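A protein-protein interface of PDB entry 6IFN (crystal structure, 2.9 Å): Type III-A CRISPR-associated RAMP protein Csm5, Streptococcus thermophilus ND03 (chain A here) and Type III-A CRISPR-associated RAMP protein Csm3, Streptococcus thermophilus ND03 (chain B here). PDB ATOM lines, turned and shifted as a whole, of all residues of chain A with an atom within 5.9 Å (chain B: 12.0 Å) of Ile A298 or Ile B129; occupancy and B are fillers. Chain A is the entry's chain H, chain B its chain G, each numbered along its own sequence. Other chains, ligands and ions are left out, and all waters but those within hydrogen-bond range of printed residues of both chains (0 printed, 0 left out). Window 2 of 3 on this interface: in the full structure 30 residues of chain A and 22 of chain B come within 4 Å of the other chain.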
ATOM      1  N   GLU A 150     -20.864  -5.434  31.287  1.00  0.00           N
ATOM      2  CA  GLU A 150     -22.108  -6.207  31.552  1.00  0.00           C
ATOM      3  C   GLU A 150     -23.147  -6.328  30.437  1.00  0.00           C
ATOM      4  O   GLU A 150     -23.427  -5.361  29.734  1.00  0.00           O
ATOM      5  CB  GLU A 150     -22.860  -5.535  32.686  1.00  0.00           C
ATOM      6  CG  GLU A 150     -22.697  -6.268  33.978  1.00  0.00           C
ATOM      7  CD  GLU A 150     -23.606  -5.635  34.992  1.00  0.00           C
ATOM      8  OE1 GLU A 150     -23.818  -4.438  34.885  1.00  0.00           O
ATOM      9  OE2 GLU A 150     -24.113  -6.346  35.855  1.00  0.00           O
ATOM     10  N   ASN A 151     -23.792  -7.497  30.481  1.00  0.00           N
ATOM     11  CA  ASN A 151     -24.910  -8.006  29.648  1.00  0.00           C
ATOM     12  C   ASN A 151     -25.769  -8.950  30.505  1.00  0.00           C
ATOM     13  O   ASN A 151     -25.330  -9.312  31.596  1.00  0.00           O
ATOM     14  CB  ASN A 151     -24.433  -8.668  28.362  1.00  0.00           C
ATOM     15  CG  ASN A 151     -23.221  -9.542  28.556  1.00  0.00           C
ATOM     16  OD1 ASN A 151     -22.242  -9.117  29.138  1.00  0.00           O
ATOM     17  ND2 ASN A 151     -23.268 -10.755  28.045  1.00  0.00           N
ATOM     18  N   PRO A 160     -27.695 -14.594  25.185  1.00  0.00           N
ATOM     19  CA  PRO A 160     -27.392 -13.334  25.870  1.00  0.00           C
ATOM     20  C   PRO A 160     -27.944 -12.073  25.189  1.00  0.00           C
ATOM     21  O   PRO A 160     -28.288 -12.097  24.006  1.00  0.00           O
ATOM     22  CB  PRO A 160     -25.855 -13.294  25.868  1.00  0.00           C
ATOM     23  CG  PRO A 160     -25.460 -14.737  25.722  1.00  0.00           C
ATOM     24  CD  PRO A 160     -26.475 -15.278  24.740  1.00  0.00           C
ATOM     25  N   LYS A 161     -27.967 -10.979  25.951  1.00  0.00           N
ATOM     26  CA  LYS A 161     -28.454  -9.671  25.465  1.00  0.00           C
ATOM     27  C   LYS A 161     -27.883  -8.553  26.336  1.00  0.00           C
ATOM     28  O   LYS A 161     -27.310  -8.853  27.370  1.00  0.00           O
ATOM     29  CB  LYS A 161     -29.957  -9.655  25.449  1.00  0.00           C
ATOM     30  N   GLU A 162     -28.067  -7.306  25.906  1.00  0.00           N
ATOM     31  CA  GLU A 162     -27.588  -6.095  26.619  1.00  0.00           C
ATOM     32  C   GLU A 162     -28.278  -6.022  27.976  1.00  0.00           C
ATOM     33  O   GLU A 162     -29.457  -6.346  28.045  1.00  0.00           O
ATOM     34  CB  GLU A 162     -27.935  -4.855  25.805  1.00  0.00           C
ATOM     35  CG  GLU A 162     -26.970  -3.719  26.031  1.00  0.00           C
ATOM     36  CD  GLU A 162     -27.308  -2.433  25.310  1.00  0.00           C
ATOM     37  OE1 GLU A 162     -26.989  -1.379  25.836  1.00  0.00           O
ATOM     38  OE2 GLU A 162     -27.887  -2.499  24.231  1.00  0.00           O
ATOM     39  N   ASN A 163     -27.590  -5.536  29.002  1.00  0.00           N
ATOM     40  CA  ASN A 163     -28.202  -5.543  30.350  1.00  0.00           C
ATOM     41  C   ASN A 163     -29.472  -4.700  30.382  1.00  0.00           C
ATOM     42  O   ASN A 163     -30.339  -5.032  31.194  1.00  0.00           O
ATOM     43  CB  ASN A 163     -27.233  -5.093  31.432  1.00  0.00           C
ATOM     44  CG  ASN A 163     -27.943  -4.893  32.744  1.00  0.00           C
ATOM     45  OD1 ASN A 163     -28.742  -3.983  32.879  1.00  0.00           O
ATOM     46  ND2 ASN A 163     -27.674  -5.751  33.703  1.00  0.00           N
ATOM     47  N   THR A 290     -21.224  -1.759  18.712  1.00  0.00           N
ATOM     48  CA  THR A 290     -21.287  -2.561  19.949  1.00  0.00           C
ATOM     49  C   THR A 290     -20.321  -2.013  21.021  1.00  0.00           C
ATOM     50  O   THR A 290     -19.581  -1.033  20.838  1.00  0.00           O
ATOM     51  CB  THR A 290     -20.988  -4.037  19.643  1.00  0.00           C
ATOM     52  OG1 THR A 290     -19.889  -4.066  18.737  1.00  0.00           O
ATOM     53  CG2 THR A 290     -22.142  -4.791  19.013  1.00  0.00           C
ATOM     54  N   LEU A 291     -20.370  -2.643  22.194  1.00  0.00           N
ATOM     55  CA  LEU A 291     -19.235  -2.724  23.074  1.00  0.00           C
ATOM     56  C   LEU A 291     -18.418  -3.921  22.609  1.00  0.00           C
ATOM     57  O   LEU A 291     -18.739  -5.045  22.989  1.00  0.00           O
ATOM     58  CB  LEU A 291     -19.698  -2.965  24.510  1.00  0.00           C
ATOM     59  CG  LEU A 291     -20.426  -1.799  25.155  1.00  0.00           C
ATOM     60  CD1 LEU A 291     -20.705  -2.075  26.627  1.00  0.00           C
ATOM     61  CD2 LEU A 291     -19.619  -0.527  24.974  1.00  0.00           C
ATOM     62  N   GLN A 294     -16.866  -6.603  25.130  1.00  0.00           N
ATOM     63  CA  GLN A 294     -17.815  -7.593  25.722  1.00  0.00           C
ATOM     64  C   GLN A 294     -18.652  -8.316  24.654  1.00  0.00           C
ATOM     65  O   GLN A 294     -19.281  -9.330  24.943  1.00  0.00           O
ATOM     66  CB  GLN A 294     -18.795  -6.928  26.682  1.00  0.00           C
ATOM     67  CG  GLN A 294     -18.172  -5.849  27.545  1.00  0.00           C
ATOM     68  CD  GLN A 294     -17.228  -6.437  28.558  1.00  0.00           C
ATOM     69  OE1 GLN A 294     -17.613  -7.319  29.329  1.00  0.00           O
ATOM     70  NE2 GLN A 294     -15.999  -5.935  28.560  1.00  0.00           N
ATOM     71  N   ALA A 295     -18.688  -7.789  23.428  1.00  0.00           N
ATOM     72  CA  ALA A 295     -19.541  -8.370  22.409  1.00  0.00           C
ATOM     73  C   ALA A 295     -18.901  -9.618  21.800  1.00  0.00           C
ATOM     74  O   ALA A 295     -19.614 -10.429  21.239  1.00  0.00           O
ATOM     75  CB  ALA A 295     -19.850  -7.358  21.335  1.00  0.00           C
ATOM     76  N   ASP A 296     -17.576  -9.751  21.918  1.00  0.00           N
ATOM     77  CA  ASP A 296     -16.760 -10.636  21.074  1.00  0.00           C
ATOM     78  C   ASP A 296     -17.341 -12.060  20.960  1.00  0.00           C
ATOM     79  O   ASP A 296     -17.887 -12.432  19.900  1.00  0.00           O
ATOM     80  CB  ASP A 296     -15.326 -10.660  21.586  1.00  0.00           C
ATOM     81  CG  ASP A 296     -14.358 -11.067  20.506  1.00  0.00           C
ATOM     82  OD1 ASP A 296     -14.794 -11.764  19.557  1.00  0.00           O
ATOM     83  OD2 ASP A 296     -13.188 -10.661  20.623  1.00  0.00           O
ATOM     84  N   GLY A 297     -17.212 -12.869  22.020  1.00  0.00           N
ATOM     85  CA  GLY A 297     -17.615 -14.294  21.988  1.00  0.00           C
ATOM     86  C   GLY A 297     -19.035 -14.486  21.468  1.00  0.00           C
ATOM     87  O   GLY A 297     -19.289 -15.355  20.604  1.00  0.00           O
ATOM     88  N   ILE A 298     -19.931 -13.607  21.949  1.00  0.00           N
ATOM     89  CA  ILE A 298     -21.398 -13.706  21.810  1.00  0.00           C
ATOM     90  C   ILE A 298     -21.811 -13.405  20.364  1.00  0.00           C
ATOM     91  O   ILE A 298     -22.538 -14.170  19.734  1.00  0.00           O
ATOM     92  CB  ILE A 298     -22.082 -12.758  22.815  1.00  0.00           C
ATOM     93  CG1 ILE A 298     -21.486 -12.914  24.222  1.00  0.00           C
ATOM     94  CG2 ILE A 298     -23.593 -12.958  22.808  1.00  0.00           C
ATOM     95  CD1 ILE A 298     -21.781 -11.769  25.153  1.00  0.00           C
ATOM     96  N   LEU A 299     -21.326 -12.285  19.838  1.00  0.00           N
ATOM     97  CA  LEU A 299     -21.645 -11.883  18.488  1.00  0.00           C
ATOM     98  C   LEU A 299     -21.312 -13.015  17.507  1.00  0.00           C
ATOM     99  O   LEU A 299     -22.164 -13.430  16.718  1.00  0.00           O
ATOM    100  CB  LEU A 299     -20.852 -10.618  18.159  1.00  0.00           C
ATOM    101  CG  LEU A 299     -21.181  -9.928  16.830  1.00  0.00           C
ATOM    102  CD1 LEU A 299     -22.548 -10.309  16.271  1.00  0.00           C
ATOM    103  CD2 LEU A 299     -21.078  -8.420  17.001  1.00  0.00           C
ATOM    104  N   GLN A 300     -20.074 -13.521  17.572  1.00  0.00           N
ATOM    105  CA  GLN A 300     -19.641 -14.628  16.706  1.00  0.00           C
ATOM    106  C   GLN A 300     -20.690 -15.743  16.782  1.00  0.00           C
ATOM    107  O   GLN A 300     -21.270 -16.113  15.772  1.00  0.00           O
ATOM    108  CB  GLN A 300     -18.257 -15.130  17.124  1.00  0.00           C
ATOM    109  CG  GLN A 300     -17.101 -14.363  16.489  1.00  0.00           C
ATOM    110  CD  GLN A 300     -16.910 -12.974  17.049  1.00  0.00           C
ATOM    111  OE1 GLN A 300     -17.872 -12.247  17.278  1.00  0.00           O
ATOM    112  NE2 GLN A 300     -15.661 -12.594  17.273  1.00  0.00           N
ATOM    113  N   ARG A 301     -20.960 -16.211  18.011  1.00  0.00           N
ATOM    114  CA  ARG A 301     -21.902 -17.298  18.284  1.00  0.00           C
ATOM    115  C   ARG A 301     -23.229 -17.053  17.551  1.00  0.00           C
ATOM    116  O   ARG A 301     -23.969 -17.986  17.299  1.00  0.00           O
ATOM    117  CB  ARG A 301     -22.151 -17.457  19.788  1.00  0.00           C
ATOM    118  CG  ARG A 301     -20.971 -18.026  20.569  1.00  0.00           C
ATOM    119  CD  ARG A 301     -21.364 -18.709  21.878  1.00  0.00           C
ATOM    120  NE  ARG A 301     -21.206 -17.887  23.084  1.00  0.00           N
ATOM    121  CZ  ARG A 301     -22.204 -17.375  23.815  1.00  0.00           C
ATOM    122  NH1 ARG A 301     -23.467 -17.549  23.459  1.00  0.00           N
ATOM    123  NH2 ARG A 301     -21.930 -16.686  24.909  1.00  0.00           N
ATOM    124  N   ARG A 302     -23.536 -15.799  17.204  1.00  0.00           N
ATOM    125  CA  ARG A 302     -24.813 -15.505  16.559  1.00  0.00           C
ATOM    126  C   ARG A 302     -24.819 -16.087  15.138  1.00  0.00           C
ATOM    127  O   ARG A 302     -25.875 -16.441  14.661  1.00  0.00           O
ATOM    128  CB  ARG A 302     -25.148 -14.002  16.571  1.00  0.00           C
ATOM    129  CG  ARG A 302     -26.611 -13.683  16.872  1.00  0.00           C
ATOM    130  CD  ARG A 302     -26.973 -12.198  16.923  1.00  0.00           C
ATOM    131  NE  ARG A 302     -27.603 -11.705  15.699  1.00  0.00           N
ATOM    132  CZ  ARG A 302     -27.459 -10.475  15.197  1.00  0.00           C
ATOM    133  NH1 ARG A 302     -28.020 -10.151  14.048  1.00  0.00           N
ATOM    134  NH2 ARG A 302     -26.749  -9.556  15.825  1.00  0.00           N
ATOM    135  N   TYR A 303     -23.658 -16.208  14.475  1.00  0.00           N
ATOM    136  CA  TYR A 303     -23.634 -16.544  13.013  1.00  0.00           C
ATOM    137  C   TYR A 303     -23.146 -17.978  12.710  1.00  0.00           C
ATOM    138  O   TYR A 303     -22.898 -18.319  11.542  1.00  0.00           O
ATOM    139  CB  TYR A 303     -22.839 -15.470  12.265  1.00  0.00           C
ATOM    140  CG  TYR A 303     -23.483 -14.111  12.358  1.00  0.00           C
ATOM    141  CD1 TYR A 303     -24.698 -13.871  11.734  1.00  0.00           C
ATOM    142  CD2 TYR A 303     -22.918 -13.091  13.113  1.00  0.00           C
ATOM    143  CE1 TYR A 303     -25.320 -12.640  11.822  1.00  0.00           C
ATOM    144  CE2 TYR A 303     -23.537 -11.856  13.221  1.00  0.00           C
ATOM    145  CZ  TYR A 303     -24.745 -11.635  12.580  1.00  0.00           C
ATOM    146  OH  TYR A 303     -25.362 -10.428  12.669  1.00  0.00           O
ATOM    147  N   THR B 125     -33.034   0.578  17.365  1.00  0.00           N
ATOM    148  CA  THR B 125     -32.071   0.484  18.414  1.00  0.00           C
ATOM    149  C   THR B 125     -31.246  -0.773  18.161  1.00  0.00           C
ATOM    150  O   THR B 125     -31.781  -1.804  17.765  1.00  0.00           O
ATOM    151  CB  THR B 125     -32.751   0.452  19.788  1.00  0.00           C
ATOM    152  OG1 THR B 125     -31.764   0.820  20.754  1.00  0.00           O
ATOM    153  CG2 THR B 125     -33.371  -0.888  20.117  1.00  0.00           C
ATOM    154  N   ILE B 126     -29.942  -0.667  18.380  1.00  0.00           N
ATOM    155  CA  ILE B 126     -29.049  -1.770  18.100  1.00  0.00           C
ATOM    156  C   ILE B 126     -28.479  -2.248  19.428  1.00  0.00           C
ATOM    157  O   ILE B 126     -27.832  -1.479  20.139  1.00  0.00           O
ATOM    158  CB  ILE B 126     -27.927  -1.375  17.122  1.00  0.00           C
ATOM    159  CG1 ILE B 126     -28.388  -0.382  16.053  1.00  0.00           C
ATOM    160  CG2 ILE B 126     -27.345  -2.637  16.516  1.00  0.00           C
ATOM    161  CD1 ILE B 126     -27.256   0.341  15.389  1.00  0.00           C
ATOM    162  N   ASP B 127     -28.769  -3.500  19.760  1.00  0.00           N
ATOM    163  CA  ASP B 127     -28.231  -4.088  20.958  1.00  0.00           C
ATOM    164  C   ASP B 127     -26.701  -4.009  20.875  1.00  0.00           C
ATOM    165  O   ASP B 127     -26.116  -4.317  19.859  1.00  0.00           O
ATOM    166  CB  ASP B 127     -28.720  -5.529  21.142  1.00  0.00           C
ATOM    167  CG  ASP B 127     -28.300  -6.129  22.465  1.00  0.00           C
ATOM    168  OD1 ASP B 127     -27.115  -6.079  22.730  1.00  0.00           O
ATOM    169  OD2 ASP B 127     -29.166  -6.604  23.232  1.00  0.00           O
ATOM    170  N   ARG B 128     -26.059  -3.585  21.962  1.00  0.00           N
ATOM    171  CA  ARG B 128     -24.626  -3.344  21.954  1.00  0.00           C
ATOM    172  C   ARG B 128     -23.843  -4.623  22.279  1.00  0.00           C
ATOM    173  O   ARG B 128     -22.632  -4.641  22.117  1.00  0.00           O
ATOM    174  CB  ARG B 128     -24.275  -2.215  22.922  1.00  0.00           C
ATOM    175  CG  ARG B 128     -24.942  -0.890  22.584  1.00  0.00           C
ATOM    176  CD  ARG B 128     -24.300  -0.181  21.413  1.00  0.00           C
ATOM    177  NE  ARG B 128     -25.228   0.727  20.756  1.00  0.00           N
ATOM    178  CZ  ARG B 128     -25.508   1.959  21.173  1.00  0.00           C
ATOM    179  NH1 ARG B 128     -25.237   2.324  22.417  1.00  0.00           N
ATOM    180  NH2 ARG B 128     -26.025   2.837  20.332  1.00  0.00           N
ATOM    181  N   ILE B 129     -24.504  -5.677  22.753  1.00  0.00           N
ATOM    182  CA  ILE B 129     -23.846  -6.965  22.980  1.00  0.00           C
ATOM    183  C   ILE B 129     -24.157  -7.932  21.826  1.00  0.00           C
ATOM    184  O   ILE B 129     -23.276  -8.611  21.362  1.00  0.00           O
ATOM    185  CB  ILE B 129     -24.213  -7.538  24.361  1.00  0.00           C
ATOM    186  CG1 ILE B 129     -23.729  -6.596  25.465  1.00  0.00           C
ATOM    187  CG2 ILE B 129     -23.683  -8.955  24.522  1.00  0.00           C
ATOM    188  CD1 ILE B 129     -22.245  -6.662  25.720  1.00  0.00           C
ATOM    189  N   THR B 130     -25.413  -8.012  21.385  1.00  0.00           N
ATOM    190  CA  THR B 130     -25.800  -9.019  20.386  1.00  0.00           C
ATOM    191  C   THR B 130     -25.776  -8.417  18.975  1.00  0.00           C
ATOM    192  O   THR B 130     -25.824  -9.154  18.019  1.00  0.00           O
ATOM    193  CB  THR B 130     -27.174  -9.625  20.696  1.00  0.00           C
ATOM    194  N   ALA B 131     -25.717  -7.084  18.857  1.00  0.00           N
ATOM    195  CA  ALA B 131     -25.758  -6.377  17.562  1.00  0.00           C
ATOM    196  C   ALA B 131     -27.131  -6.513  16.886  1.00  0.00           C
ATOM    197  O   ALA B 131     -27.289  -6.141  15.719  1.00  0.00           O
ATOM    198  CB  ALA B 131     -24.672  -6.888  16.658  1.00  0.00           C
ATOM    199  N   GLU B 132     -28.120  -7.047  17.609  1.00  0.00           N
ATOM    200  CA  GLU B 132     -29.472  -7.234  17.042  1.00  0.00           C
ATOM    201  C   GLU B 132     -30.160  -5.875  16.988  1.00  0.00           C
ATOM    202  O   GLU B 132     -30.033  -5.090  17.912  1.00  0.00           O
ATOM    203  CB  GLU B 132     -30.286  -8.246  17.855  1.00  0.00           C
ATOM    204  CG  GLU B 132     -29.773  -9.676  17.713  1.00  0.00           C
ATOM    205  CD  GLU B 132     -30.198 -10.647  18.802  1.00  0.00           C
ATOM    206  OE1 GLU B 132     -30.552 -11.803  18.466  1.00  0.00           O
ATOM    207  OE2 GLU B 132     -30.139 -10.247  19.985  1.00  0.00           O
ATOM    208  N   ALA B 133     -30.917  -5.637  15.915  1.00  0.00           N
ATOM    209  CA  ALA B 133     -31.580  -4.349  15.686  1.00  0.00           C
ATOM    210  C   ALA B 133     -33.095  -4.509  15.849  1.00  0.00           C
ATOM    211  O   ALA B 133     -33.692  -5.422  15.290  1.00  0.00           O
ATOM    212  CB  ALA B 133     -31.229  -3.831  14.315  1.00  0.00           C
ATOM    213  N   ASN B 134     -33.709  -3.627  16.631  1.00  0.00           N
ATOM    214  CA  ASN B 134     -35.148  -3.657  16.809  1.00  0.00           C
ATOM    215  C   ASN B 134     -35.719  -2.352  16.278  1.00  0.00           C
ATOM    216  O   ASN B 134     -35.472  -1.285  16.836  1.00  0.00           O
ATOM    217  CB  ASN B 134     -35.551  -3.902  18.265  1.00  0.00           C
ATOM    218  CG  ASN B 134     -36.738  -4.829  18.347  1.00  0.00           C
ATOM    219  OD1 ASN B 134     -36.548  -6.030  18.570  1.00  0.00           O
ATOM    220  ND2 ASN B 134     -37.941  -4.294  18.166  1.00  0.00           N
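Of the 18 printed residues of chain A, 10 touch a printed residue of chain B. Of the 10 printed residues of chain B, 6 touch a printed residue of chain A. Printed residues of chain B that touch a printed residue of chain A: Asp B127, Arg B128, Ile B129, Thr B130, Ala B131 and Glu B132. Among the printed residues, 15 pairs touch across the chains. Among the printed residues, no Asp or Glu carboxylate lies within 4 Å of a Lys or Arg side-chain nitrogen of the other chain.
Among the printed residues, merely in contact across the chains: Thr A290 with Arg B128 (3.0 Å), Ile A298 with Ile B129 (3.5 Å), Gln A294 with Ile B129 (3.6 Å), Asn A151 with Ile B129 (3.6 Å), Ala A295 with Ile B129 (3.6 Å), Lys A161 with Asp B127 (3.9 Å), Leu A299 with Thr B130 (3.9 Å), Leu A299 with Ala B131 (3.9 Å) and Ala A295 with Arg B128 (3.97 Å).
NH1 of Arg A302 is in hydrogen-bond range of OH of Tyr A303, 3.0 Å away. OD1 of Asp B127 is in hydrogen-bond range of N of Ile B129 (2.6 Å). The side-chain carboxylate (OD1) of Asp B127 lies within hydrogen-bond range of the backbone NH (N) of Thr B130 (2.9 Å). The guanidinium group of Arg B128 sits at hydrogen-bond distance from the backbone carbonyl oxygen of Ile B126. The backbone NH (N) of Asp B127 is in hydrogen-bond range of the backbone carbonyl oxygen (O) of Glu B132.
Glu A150 touches none of the printed residues of chain B. No residue of chain B comes within 4 Å of Pro A160. Of chain B, only Asp B127 (3.9 Å) comes within 4 Å of Lys A161. Glu A162 touches just these residues of chain B: Asp B127 (3.0 Å) and Arg B128 (3.1 Å). Of chain B, only Arg B128 (3.0 Å) comes within 4 Å of Thr A290. Of chain B, only Arg B128 comes within 4 Å of Leu A291. Gln A294 touches just one residue of chain B: Ile B129 (3.6 Å). No residue of chain B comes within 4 Å of Asp A296. Of chain B, only Ile B129 comes within 4 Å of Ile A298. No residue of chain B comes within 4 Å of Gln A300. Printed residues of chain A within 4 Å of Asp B127: Lys A161 (3.9 Å) and Glu A162 (3.0 Å). Of the printed residues of chain A, Arg B128 touches Glu A162 (3.1 Å), Thr A290 (3.0 Å), Leu A291 (3.0 Å) and Ala A295 (3.97 Å). Of chain A, only Asn A151, Gln A294, Ala A295 and Ile A298 come within 4 Å of Ile B129. Of the printed residues of chain A, Thr B130 touches Leu A299 and Arg A302. Of the printed residues of chain A, Ala B131 touches Leu A299 (3.9 Å) and Arg A302 (3.2 Å). Of the printed residues of chain A, Glu B132 touches Arg A302 (3.4 Å). The nearest residue of chain B that does not touch Ile A298 is Thr B130 (5.1 Å). The nearest residue of chain A that does not touch Ile B129 is Glu A162 (4.1 Å).
The backbone NH (N) of Arg B128 lies within hydrogen-bond range of the side-chain carboxylate (OE2) of Glu A162 (3.1 Å). O of Arg B128 lies within hydrogen-bond range of N of Leu A291 (3.0 Å). NH2 of Arg A302 lies close to O of Ala B131. The backbone carbonyl oxygen (O) of Thr B130 lies within hydrogen-bond range of the guanidinium group (NH2) of Arg A302. The guanidinium group (NH2) of Arg A302 sits close to the backbone NH (N) of Glu B132, 3.4 Å away. The backbone NH (N) of Glu A162 sits at hydrogen-bond distance from the side-chain carboxylate (OD2) of Asp B127 (3.0 Å).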
